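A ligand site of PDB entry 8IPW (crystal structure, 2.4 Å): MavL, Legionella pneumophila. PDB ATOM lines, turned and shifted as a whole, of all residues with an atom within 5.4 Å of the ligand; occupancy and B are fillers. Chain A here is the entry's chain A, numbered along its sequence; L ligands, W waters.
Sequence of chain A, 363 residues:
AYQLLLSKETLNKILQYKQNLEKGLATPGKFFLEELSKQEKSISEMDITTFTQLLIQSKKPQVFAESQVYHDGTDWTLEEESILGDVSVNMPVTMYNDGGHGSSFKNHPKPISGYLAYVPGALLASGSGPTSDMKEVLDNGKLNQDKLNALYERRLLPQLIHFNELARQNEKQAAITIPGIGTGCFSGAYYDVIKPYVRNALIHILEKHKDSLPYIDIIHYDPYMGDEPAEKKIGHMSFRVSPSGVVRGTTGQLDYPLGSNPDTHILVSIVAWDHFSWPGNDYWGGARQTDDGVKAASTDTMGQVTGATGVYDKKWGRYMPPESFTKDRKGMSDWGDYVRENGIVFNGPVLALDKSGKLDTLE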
ATOM      1  N   VAL A  63       4.146  -8.087 -16.875  1.00  0.00           N
ATOM      2  CA  VAL A  63       3.727  -8.011 -15.460  1.00  0.00           C
ATOM      3  C   VAL A  63       2.655  -6.953 -15.392  1.00  0.00           C
ATOM      4  O   VAL A  63       2.867  -5.857 -15.885  1.00  0.00           O
ATOM      5  CB  VAL A  63       4.834  -7.547 -14.471  1.00  0.00           C
ATOM      6  CG1 VAL A  63       4.370  -7.694 -13.023  1.00  0.00           C
ATOM      7  CG2 VAL A  63       6.162  -8.249 -14.695  1.00  0.00           C
ATOM      8  N   PHE A  64       1.557  -7.219 -14.732  1.00  0.00           N
ATOM      9  CA  PHE A  64       0.523  -6.210 -14.498  1.00  0.00           C
ATOM     10  C   PHE A  64       0.752  -5.723 -13.070  1.00  0.00           C
ATOM     11  O   PHE A  64       0.345  -6.391 -12.138  1.00  0.00           O
ATOM     12  CB  PHE A  64      -0.865  -6.847 -14.645  1.00  0.00           C
ATOM     13  CG  PHE A  64      -1.261  -7.096 -16.085  1.00  0.00           C
ATOM     14  CD1 PHE A  64      -1.159  -6.088 -17.038  1.00  0.00           C
ATOM     15  CD2 PHE A  64      -1.748  -8.336 -16.481  1.00  0.00           C
ATOM     16  CE1 PHE A  64      -1.563  -6.314 -18.344  1.00  0.00           C
ATOM     17  CE2 PHE A  64      -2.107  -8.556 -17.800  1.00  0.00           C
ATOM     18  CZ  PHE A  64      -2.037  -7.548 -18.725  1.00  0.00           C
ATOM     19  N   ALA A  65       1.482  -4.589 -12.890  1.00  0.00           N
ATOM     20  CA  ALA A  65       1.840  -4.029 -11.573  1.00  0.00           C
ATOM     21  C   ALA A  65       0.651  -3.760 -10.645  1.00  0.00           C
ATOM     22  O   ALA A  65       0.784  -3.846  -9.421  1.00  0.00           O
ATOM     23  CB  ALA A  65       2.658  -2.741 -11.749  1.00  0.00           C
ATOM     24  N   GLU A  66      -0.478  -3.387 -11.219  1.00  0.00           N
ATOM     25  CA  GLU A  66      -1.653  -3.054 -10.439  1.00  0.00           C
ATOM     26  C   GLU A  66      -2.377  -4.262  -9.854  1.00  0.00           C
ATOM     27  O   GLU A  66      -3.198  -4.063  -8.973  1.00  0.00           O
ATOM     28  CB  GLU A  66      -2.626  -2.181 -11.255  1.00  0.00           C
ATOM     29  CG  GLU A  66      -3.435  -2.940 -12.275  1.00  0.00           C
ATOM     30  CD  GLU A  66      -2.753  -3.335 -13.575  1.00  0.00           C
ATOM     31  OE1 GLU A  66      -3.360  -4.143 -14.321  1.00  0.00           O
ATOM     32  OE2 GLU A  66      -1.636  -2.827 -13.859  1.00  0.00           O
ATOM     33  N   HIS A 101      -5.779   3.288 -31.174  1.00  0.00           N
ATOM     34  CA  HIS A 101      -6.062   1.987 -30.579  1.00  0.00           C
ATOM     35  C   HIS A 101      -7.063   1.204 -31.443  1.00  0.00           C
ATOM     36  O   HIS A 101      -7.743   1.805 -32.283  1.00  0.00           O
ATOM     37  CB  HIS A 101      -6.540   2.130 -29.114  1.00  0.00           C
ATOM     38  CG  HIS A 101      -5.499   2.646 -28.160  1.00  0.00           C
ATOM     39  ND1 HIS A 101      -5.404   2.181 -26.872  1.00  0.00           N
ATOM     40  CD2 HIS A 101      -4.531   3.585 -28.346  1.00  0.00           C
ATOM     41  CE1 HIS A 101      -4.411   2.842 -26.293  1.00  0.00           C
ATOM     42  NE2 HIS A 101      -3.846   3.694 -27.146  1.00  0.00           N
ATOM     43  N   GLY A 121       3.617   5.688 -14.422  1.00  0.00           N
ATOM     44  CA  GLY A 121       2.805   6.641 -13.682  1.00  0.00           C
ATOM     45  C   GLY A 121       2.578   6.180 -12.261  1.00  0.00           C
ATOM     46  O   GLY A 121       3.038   5.108 -11.836  1.00  0.00           O
ATOM     47  N   PRO A 179       0.344  10.917 -23.205  1.00  0.00           N
ATOM     48  CA  PRO A 179      -1.001  10.364 -22.971  1.00  0.00           C
ATOM     49  C   PRO A 179      -1.444  10.637 -21.520  1.00  0.00           C
ATOM     50  O   PRO A 179      -0.739  11.299 -20.756  1.00  0.00           O
ATOM     51  CB  PRO A 179      -0.770   8.872 -23.207  1.00  0.00           C
ATOM     52  CG  PRO A 179       0.666   8.644 -22.663  1.00  0.00           C
ATOM     53  CD  PRO A 179       1.398   9.951 -22.843  1.00  0.00           C
ATOM     54  N   GLY A 180      -2.609  10.103 -21.117  1.00  0.00           N
ATOM     55  CA  GLY A 180      -3.115  10.267 -19.761  1.00  0.00           C
ATOM     56  C   GLY A 180      -2.466   9.251 -18.860  1.00  0.00           C
ATOM     57  O   GLY A 180      -3.107   8.288 -18.405  1.00  0.00           O
ATOM     58  N   ILE A 181      -1.167   9.438 -18.632  1.00  0.00           N
ATOM     59  CA  ILE A 181      -0.319   8.575 -17.824  1.00  0.00           C
ATOM     60  C   ILE A 181      -0.845   8.433 -16.394  1.00  0.00           C
ATOM     61  O   ILE A 181      -1.037   9.431 -15.685  1.00  0.00           O
ATOM     62  CB  ILE A 181       1.158   9.073 -17.900  1.00  0.00           C
ATOM     63  CG1 ILE A 181       2.066   8.305 -16.963  1.00  0.00           C
ATOM     64  CG2 ILE A 181       1.270  10.598 -17.663  1.00  0.00           C
ATOM     65  CD1 ILE A 181       3.589   8.669 -17.173  1.00  0.00           C
ATOM     66  N   GLY A 182      -1.093   7.199 -15.978  1.00  0.00           N
ATOM     67  CA  GLY A 182      -1.603   6.950 -14.640  1.00  0.00           C
ATOM     68  C   GLY A 182      -3.078   7.225 -14.460  1.00  0.00           C
ATOM     69  O   GLY A 182      -3.602   7.119 -13.347  1.00  0.00           O
ATOM     70  N   THR A 183      -3.793   7.544 -15.552  1.00  0.00           N
ATOM     71  CA  THR A 183      -5.221   7.855 -15.481  1.00  0.00           C
ATOM     72  C   THR A 183      -6.152   6.703 -15.812  1.00  0.00           C
ATOM     73  O   THR A 183      -7.358   6.886 -15.752  1.00  0.00           O
ATOM     74  CB  THR A 183      -5.553   9.070 -16.345  1.00  0.00           C
ATOM     75  OG1 THR A 183      -5.415   8.708 -17.722  1.00  0.00           O
ATOM     76  CG2 THR A 183      -4.693  10.257 -16.023  1.00  0.00           C
ATOM     77  N   GLY A 184      -5.623   5.538 -16.174  1.00  0.00           N
ATOM     78  CA  GLY A 184      -6.457   4.397 -16.511  1.00  0.00           C
ATOM     79  C   GLY A 184      -6.316   3.282 -15.499  1.00  0.00           C
ATOM     80  O   GLY A 184      -6.749   3.417 -14.356  1.00  0.00           O
ATOM     81  N   CYS A 185      -5.656   2.183 -15.915  1.00  0.00           N
ATOM     82  CA  CYS A 185      -5.410   1.026 -15.043  1.00  0.00           C
ATOM     83  C   CYS A 185      -4.743   1.406 -13.720  1.00  0.00           C
ATOM     84  O   CYS A 185      -5.125   0.895 -12.682  1.00  0.00           O
ATOM     85  CB  CYS A 185      -4.597  -0.031 -15.783  1.00  0.00           C
ATOM     86  SG  CYS A 185      -5.453  -0.744 -17.221  1.00  0.00           S
ATOM     87  N   PHE A 186      -3.730   2.274 -13.777  1.00  0.00           N
ATOM     88  CA  PHE A 186      -2.982   2.656 -12.578  1.00  0.00           C
ATOM     89  C   PHE A 186      -3.714   3.601 -11.600  1.00  0.00           C
ATOM     90  O   PHE A 186      -3.232   3.791 -10.508  1.00  0.00           O
ATOM     91  CB  PHE A 186      -1.613   3.281 -12.958  1.00  0.00           C
ATOM     92  CG  PHE A 186      -0.464   2.327 -13.187  1.00  0.00           C
ATOM     93  CD1 PHE A 186      -0.683   0.983 -13.408  1.00  0.00           C
ATOM     94  CD2 PHE A 186       0.852   2.780 -13.191  1.00  0.00           C
ATOM     95  CE1 PHE A 186       0.387   0.110 -13.631  1.00  0.00           C
ATOM     96  CE2 PHE A 186       1.916   1.913 -13.412  1.00  0.00           C
ATOM     97  CZ  PHE A 186       1.672   0.583 -13.618  1.00  0.00           C
ATOM     98  N   SER A 187      -4.849   4.192 -11.971  1.00  0.00           N
ATOM     99  CA  SER A 187      -5.566   5.123 -11.096  1.00  0.00           C
ATOM    100  C   SER A 187      -6.399   4.460 -10.001  1.00  0.00           C
ATOM    101  O   SER A 187      -6.816   5.134  -9.066  1.00  0.00           O
ATOM    102  CB  SER A 187      -6.425   6.091 -11.896  1.00  0.00           C
ATOM    103  OG  SER A 187      -7.441   5.373 -12.568  1.00  0.00           O
ATOM    104  N   LYS A 195      -7.931  12.489 -13.704  1.00  0.00           N
ATOM    105  CA  LYS A 195      -7.566  13.271 -14.893  1.00  0.00           C
ATOM    106  C   LYS A 195      -7.129  14.728 -14.600  1.00  0.00           C
ATOM    107  O   LYS A 195      -6.018  15.073 -15.004  1.00  0.00           O
ATOM    108  CB  LYS A 195      -8.666  13.220 -15.961  1.00  0.00           C
ATOM    109  CG  LYS A 195      -9.044  11.814 -16.338  1.00  0.00           C
ATOM    110  CD  LYS A 195      -8.436  11.333 -17.650  1.00  0.00           C
ATOM    111  CE  LYS A 195      -9.149  10.056 -18.073  1.00  0.00           C
ATOM    112  NZ  LYS A 195      -8.647   9.497 -19.345  1.00  0.00           N
ATOM    113  N   ASP A 222      -2.878  14.343 -24.690  1.00  0.00           N
ATOM    114  CA  ASP A 222      -4.125  13.683 -25.110  1.00  0.00           C
ATOM    115  C   ASP A 222      -4.556  12.666 -24.042  1.00  0.00           C
ATOM    116  O   ASP A 222      -4.106  11.533 -24.049  1.00  0.00           O
ATOM    117  CB  ASP A 222      -3.945  13.010 -26.490  1.00  0.00           C
ATOM    118  CG  ASP A 222      -5.132  12.224 -27.059  1.00  0.00           C
ATOM    119  OD1 ASP A 222      -6.159  12.116 -26.358  1.00  0.00           O
ATOM    120  OD2 ASP A 222      -5.037  11.736 -28.211  1.00  0.00           O
ATOM    121  N   PRO A 223      -5.475  13.067 -23.134  1.00  0.00           N
ATOM    122  CA  PRO A 223      -5.953  12.115 -22.123  1.00  0.00           C
ATOM    123  C   PRO A 223      -7.131  11.245 -22.582  1.00  0.00           C
ATOM    124  O   PRO A 223      -7.790  10.645 -21.741  1.00  0.00           O
ATOM    125  CB  PRO A 223      -6.383  13.023 -20.972  1.00  0.00           C
ATOM    126  CG  PRO A 223      -6.782  14.303 -21.630  1.00  0.00           C
ATOM    127  CD  PRO A 223      -6.085  14.399 -22.966  1.00  0.00           C
ATOM    128  N   TYR A 224      -7.436  11.204 -23.912  1.00  0.00           N
ATOM    129  CA  TYR A 224      -8.532  10.464 -24.549  1.00  0.00           C
ATOM    130  C   TYR A 224      -9.924  11.064 -24.203  1.00  0.00           C
ATOM    131  O   TYR A 224     -10.629  11.513 -25.096  1.00  0.00           O
ATOM    132  CB  TYR A 224      -8.483   8.933 -24.329  1.00  0.00           C
ATOM    133  CG  TYR A 224      -9.452   8.214 -25.232  1.00  0.00           C
ATOM    134  CD1 TYR A 224      -9.446   8.419 -26.609  1.00  0.00           C
ATOM    135  CD2 TYR A 224     -10.411   7.359 -24.705  1.00  0.00           C
ATOM    136  CE1 TYR A 224     -10.356   7.773 -27.441  1.00  0.00           C
ATOM    137  CE2 TYR A 224     -11.319   6.700 -25.534  1.00  0.00           C
ATOM    138  CZ  TYR A 224     -11.296   6.917 -26.902  1.00  0.00           C
ATOM    139  OH  TYR A 224     -12.194   6.302 -27.742  1.00  0.00           O
ATOM    140  N   MET A 225     -10.255  11.106 -22.915  1.00  0.00           N
ATOM    141  CA  MET A 225     -11.497  11.713 -22.479  1.00  0.00           C
ATOM    142  C   MET A 225     -11.343  12.248 -21.063  1.00  0.00           C
ATOM    143  O   MET A 225     -10.304  12.070 -20.465  1.00  0.00           O
ATOM    144  CB  MET A 225     -12.636  10.699 -22.584  1.00  0.00           C
ATOM    145  CG  MET A 225     -13.592  10.987 -23.721  1.00  0.00           C
ATOM    146  SD  MET A 225     -14.917   9.785 -23.894  1.00  0.00           S
ATOM    147  CE  MET A 225     -14.388   8.880 -25.334  1.00  0.00           C
ATOM    148  N   ALA A 272       3.034   5.452 -21.173  1.00  0.00           N
ATOM    149  CA  ALA A 272       2.602   5.100 -19.830  1.00  0.00           C
ATOM    150  C   ALA A 272       3.025   3.637 -19.583  1.00  0.00           C
ATOM    151  O   ALA A 272       2.340   2.695 -19.962  1.00  0.00           O
ATOM    152  CB  ALA A 272       1.087   5.262 -19.721  1.00  0.00           C
ATOM    153  N   TRP A 273       4.191   3.495 -18.943  1.00  0.00           N
ATOM    154  CA  TRP A 273       4.910   2.261 -18.641  1.00  0.00           C
ATOM    155  C   TRP A 273       4.532   1.654 -17.267  1.00  0.00           C
ATOM    156  O   TRP A 273       3.575   2.083 -16.613  1.00  0.00           O
ATOM    157  CB  TRP A 273       6.411   2.572 -18.810  1.00  0.00           C
ATOM    158  CG  TRP A 273       7.337   1.410 -18.877  1.00  0.00           C
ATOM    159  CD1 TRP A 273       7.050   0.132 -19.232  1.00  0.00           C
ATOM    160  CD2 TRP A 273       8.719   1.435 -18.528  1.00  0.00           C
ATOM    161  NE1 TRP A 273       8.170  -0.658 -19.122  1.00  0.00           N
ATOM    162  CE2 TRP A 273       9.206   0.115 -18.667  1.00  0.00           C
ATOM    163  CE3 TRP A 273       9.593   2.428 -18.068  1.00  0.00           C
ATOM    164  CZ2 TRP A 273      10.553  -0.191 -18.494  1.00  0.00           C
ATOM    165  CZ3 TRP A 273      10.912   2.105 -17.851  1.00  0.00           C
ATOM    166  CH2 TRP A 273      11.379   0.799 -18.035  1.00  0.00           C
ATOM    167  N   ASP A 274       5.217   0.589 -16.883  1.00  0.00           N
ATOM    168  CA  ASP A 274       4.961  -0.206 -15.684  1.00  0.00           C
ATOM    169  C   ASP A 274       6.262  -0.311 -14.884  1.00  0.00           C
ATOM    170  O   ASP A 274       7.323  -0.497 -15.479  1.00  0.00           O
ATOM    171  CB  ASP A 274       4.550  -1.609 -16.144  1.00  0.00           C
ATOM    172  CG  ASP A 274       3.912  -2.517 -15.125  1.00  0.00           C
ATOM    173  OD1 ASP A 274       4.658  -3.242 -14.426  1.00  0.00           O
ATOM    174  OD2 ASP A 274       2.648  -2.569 -15.070  1.00  0.00           O
ATOM    175  N   SER A 277       7.793  -4.046 -15.590  1.00  0.00           N
ATOM    176  CA  SER A 277       7.852  -4.716 -16.884  1.00  0.00           C
ATOM    177  C   SER A 277       8.826  -4.078 -17.867  1.00  0.00           C
ATOM    178  O   SER A 277       9.233  -2.948 -17.675  1.00  0.00           O
ATOM    179  CB  SER A 277       6.451  -4.833 -17.507  1.00  0.00           C
ATOM    180  OG  SER A 277       6.129  -3.681 -18.272  1.00  0.00           O
ATOM    181  N   ASN A 281       5.371  -4.227 -22.463  1.00  0.00           N
ATOM    182  CA  ASN A 281       4.476  -4.932 -21.518  1.00  0.00           C
ATOM    183  C   ASN A 281       3.463  -5.901 -22.253  1.00  0.00           C
ATOM    184  O   ASN A 281       3.889  -6.930 -22.762  1.00  0.00           O
ATOM    185  CB  ASN A 281       3.809  -4.009 -20.474  1.00  0.00           C
ATOM    186  CG  ASN A 281       3.115  -4.754 -19.312  1.00  0.00           C
ATOM    187  OD1 ASN A 281       2.421  -4.169 -18.477  1.00  0.00           O
ATOM    188  ND2 ASN A 281       3.284  -6.038 -19.213  1.00  0.00           N
ATOM    189  N   ASP A 282       2.149  -5.602 -22.300  1.00  0.00           N
ATOM    190  CA  ASP A 282       1.161  -6.455 -22.940  1.00  0.00           C
ATOM    191  C   ASP A 282       1.547  -6.917 -24.361  1.00  0.00           C
ATOM    192  O   ASP A 282       1.219  -8.038 -24.733  1.00  0.00           O
ATOM    193  CB  ASP A 282      -0.217  -5.755 -22.962  1.00  0.00           C
ATOM    194  CG  ASP A 282      -1.357  -6.551 -22.375  1.00  0.00           C
ATOM    195  OD1 ASP A 282      -2.503  -6.018 -22.331  1.00  0.00           O
ATOM    196  OD2 ASP A 282      -1.133  -7.750 -22.002  1.00  0.00           O
ATOM    197  N   THR A 290      -2.923  -1.527 -24.512  1.00  0.00           N
ATOM    198  CA  THR A 290      -2.833  -0.324 -23.686  1.00  0.00           C
ATOM    199  C   THR A 290      -2.047   0.763 -24.397  1.00  0.00           C
ATOM    200  O   THR A 290      -1.574   0.509 -25.483  1.00  0.00           O
ATOM    201  CB  THR A 290      -2.188  -0.781 -22.370  1.00  0.00           C
ATOM    202  OG1 THR A 290      -0.895  -1.318 -22.713  1.00  0.00           O
ATOM    203  CG2 THR A 290      -3.051  -1.860 -21.653  1.00  0.00           C
ATOM    204  N   ASP A 291      -1.831   1.962 -23.785  1.00  0.00           N
ATOM    205  CA  ASP A 291      -0.962   2.981 -24.386  1.00  0.00           C
ATOM    206  C   ASP A 291       0.456   2.357 -24.579  1.00  0.00           C
ATOM    207  O   ASP A 291       0.994   2.386 -25.687  1.00  0.00           O
ATOM    208  CB  ASP A 291      -0.883   4.205 -23.464  1.00  0.00           C
ATOM    209  CG  ASP A 291       0.062   5.287 -23.963  1.00  0.00           C
ATOM    210  OD1 ASP A 291       1.231   5.326 -23.495  1.00  0.00           O
ATOM    211  OD2 ASP A 291      -0.358   6.109 -24.812  1.00  0.00           O
ATOM    212  N   ASP A 292       0.944   1.648 -23.561  1.00  0.00           N
ATOM    213  CA  ASP A 292       2.202   0.912 -23.561  1.00  0.00           C
ATOM    214  C   ASP A 292       2.313  -0.126 -24.706  1.00  0.00           C
ATOM    215  O   ASP A 292       3.303  -0.120 -25.429  1.00  0.00           O
ATOM    216  CB  ASP A 292       2.387   0.200 -22.177  1.00  0.00           C
ATOM    217  CG  ASP A 292       3.842  -0.117 -21.831  1.00  0.00           C
ATOM    218  OD1 ASP A 292       4.710   0.102 -22.677  1.00  0.00           O
ATOM    219  OD2 ASP A 292       4.098  -0.587 -20.703  1.00  0.00           O
HETATM  220  N1  LIG L   1      -7.842   4.734 -27.260  1.00  0.00           N
HETATM  221  C1  LIG L   1      -6.911   5.649 -26.897  1.00  0.00           C
HETATM  222  N2  LIG L   1      -6.689   5.892 -25.610  1.00  0.00           N
HETATM  223  C2  LIG L   1      -7.368   5.186 -24.640  1.00  0.00           C
HETATM  224  C3  LIG L   1      -8.267   4.291 -25.009  1.00  0.00           C
HETATM  225  C4  LIG L   1      -8.518   4.083 -26.341  1.00  0.00           C
HETATM  226  N3  LIG L   1      -9.386   3.211 -27.102  1.00  0.00           N
HETATM  227  N4  LIG L   1      -8.834   3.769 -23.893  1.00  0.00           N
HETATM  228  C5  LIG L   1      -8.242   4.341 -22.846  1.00  0.00           C
HETATM  229  N5  LIG L   1      -7.308   5.181 -23.292  1.00  0.00           N
HETATM  230  P1  LIG L   1      -3.419   3.119 -19.505  1.00  0.00           P
HETATM  231  P2  LIG L   1      -1.867   3.677 -16.986  1.00  0.00           P
HETATM  232  C6  LIG L   1      -6.492   6.092 -22.572  1.00  0.00           C
HETATM  233  O1  LIG L   1      -4.301   2.175 -18.733  1.00  0.00           O
HETATM  234  O2  LIG L   1      -0.701   4.563 -16.728  1.00  0.00           O
HETATM  235  C7  LIG L   1      -0.071  -0.761 -19.213  1.00  0.00           C
HETATM  236  O3  LIG L   1      -0.425  -2.067 -19.254  1.00  0.00           O
HETATM  237  C8  LIG L   1      -6.818   6.200 -21.289  1.00  0.00           C
HETATM  238  O4  LIG L   1      -7.970   7.049 -21.096  1.00  0.00           O
HETATM  239  O5  LIG L   1      -2.899   2.430 -20.713  1.00  0.00           O
HETATM  240  O6  LIG L   1      -3.036   4.117 -16.200  1.00  0.00           O
HETATM  241  C9  LIG L   1       1.195  -0.527 -18.728  1.00  0.00           C
HETATM  242  O7  LIG L   1       2.262  -1.489 -19.132  1.00  0.00           O
HETATM  243  C10 LIG L   1      -5.502   6.807 -20.590  1.00  0.00           C
HETATM  244  O8  LIG L   1      -5.622   8.235 -20.530  1.00  0.00           O
HETATM  245  O9  LIG L   1      -2.102   3.724 -18.629  1.00  0.00           O
HETATM  246  C11 LIG L   1       0.974  -0.568 -17.199  1.00  0.00           C
HETATM  247  O10 LIG L   1       0.830  -1.802 -16.748  1.00  0.00           O
HETATM  248  C12 LIG L   1      -4.412   6.435 -21.338  1.00  0.00           C
HETATM  249  O11 LIG L   1      -4.944   5.700 -22.588  1.00  0.00           O
HETATM  250  C13 LIG L   1      -0.408   0.221 -17.062  1.00  0.00           C
HETATM  251  O12 LIG L   1      -1.098   0.001 -18.158  1.00  0.00           O
HETATM  252  C14 LIG L   1      -3.467   5.559 -20.511  1.00  0.00           C
HETATM  253  O13 LIG L   1      -4.194   4.518 -19.842  1.00  0.00           O
HETATM  254  C15 LIG L   1      -0.191   1.701 -16.854  1.00  0.00           C
HETATM  255  O14 LIG L   1      -1.462   2.160 -16.551  1.00  0.00           O
HETATM  256  O   HOH W   1       1.767   4.641 -16.340  1.00  0.00           O
HETATM  257  O   HOH W   2       0.661  -3.107 -21.448  1.00  0.00           O
HETATM  258  O   HOH W   3      -0.167   2.136 -20.804  1.00  0.00           O
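Water W1 lies within hydrogen-bond range of an oxygen (O2) of the ligand (2.5 Å), the backbone NH (N) of Gly 121 (2.9 Å) and the backbone carbonyl oxygen (O) of Trp 273 (3.1 Å). Water W2 lies within hydrogen-bond range of O3 of the ligand, OG1 of Thr 290 and N of Asp 282. Water W3 lies within hydrogen-bond range of the backbone carbonyl oxygen (O) of Ala 272 (2.7 Å), an oxygen (O5) of the ligand (2.7 Å), the backbone NH (N) of Asp 292 (3.0 Å) and the backbone NH (N) of Asp 291 (3.4 Å).
O2 of the ligand sits at hydrogen-bond distance from N of Gly 182, 2.8 Å away. OD2 of Asp 292 sits at hydrogen-bond distance from O7 of the ligand, 2.6 Å away. O8 of the ligand is in hydrogen-bond range of O of Gly 180 (3.3 Å). O6 of the ligand is in hydrogen-bond range of N of Gly 184 (3.0 Å). The side-chain hydroxyl (OG1) of Thr 183 sits at hydrogen-bond distance from an oxygen (O8) of the ligand. OD2 of Asp 274 is in hydrogen-bond range of O10 of the ligand, 2.6 Å away. N of Cys 185 lies within hydrogen-bond range of O1 of the ligand, 3.1 Å away. N of Asp 291 lies within hydrogen-bond range of O5 of the ligand (3.3 Å). The backbone carbonyl oxygen (O) of Pro 223 sits at hydrogen-bond distance from an oxygen (O8) of the ligand (3.5 Å). NZ of Lys 195 sits at hydrogen-bond distance from O4 of the ligand, at 3.1 Å. An oxygen (O7) of the ligand lies within hydrogen-bond range of the side-chain amide oxygen (OD1) of Asn 281 (2.8 Å). An oxygen (O1) of the ligand is in hydrogen-bond range of the side-chain sulfur of Cys 185 (3.5 Å). O6 of the ligand sits at hydrogen-bond distance from N of Phe 186.
The side-chain amino group (NZ) of Lys 195 is in hydrogen-bond range of the backbone carbonyl oxygen (O) of Met 225, at 3.3 Å. The backbone carbonyl oxygen (O) of Val 63 sits close to the side-chain amide oxygen (OD1) of Asn 281. The backbone NH of Ala 272 is in hydrogen-bond range of the side-chain carboxylate of Asp 291, at 2.9 Å. N of Ser 277 sits at hydrogen-bond distance from OD1 of Asp 274, at 3.4 Å. OG of Ser 187 is in hydrogen-bond range of O of Gly 184 (2.7 Å). The backbone NH (N) of Tyr 224 sits at hydrogen-bond distance from the side-chain carboxylate (OD1) of Asp 222. OG1 of Thr 183 sits at hydrogen-bond distance from O of Gly 180, at 2.4 Å. O of Gly 182 lies close to N of Ser 187 (3.5 Å).
Residues that only touch the ligand: Glu 66 (3.9 Å), His 101 (3.3 Å), Ile 181 (3.9 Å), Tyr 224 (3.6 Å), Ala 272 (3.6 Å), Trp 273 (3.8 Å) and Thr 290 (3.6 Å). Hydrophobic or aromatic side chains that line the ligand: His 101, Phe 186, Tyr 224 and Ala 272. Within 4 Å of the ligand: Glu 66, His 101, Gly 180, Ile 181, Gly 182, Thr 183, Gly 184, Cys 185, Phe 186, Lys 195, Pro 223, Tyr 224, Ala 272, Trp 273, Asp 274, Asn 281, Thr 290, Asp 291 and Asp 292. Along chain A the residues within 4 Å of the ligand span positions 66 to 292.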
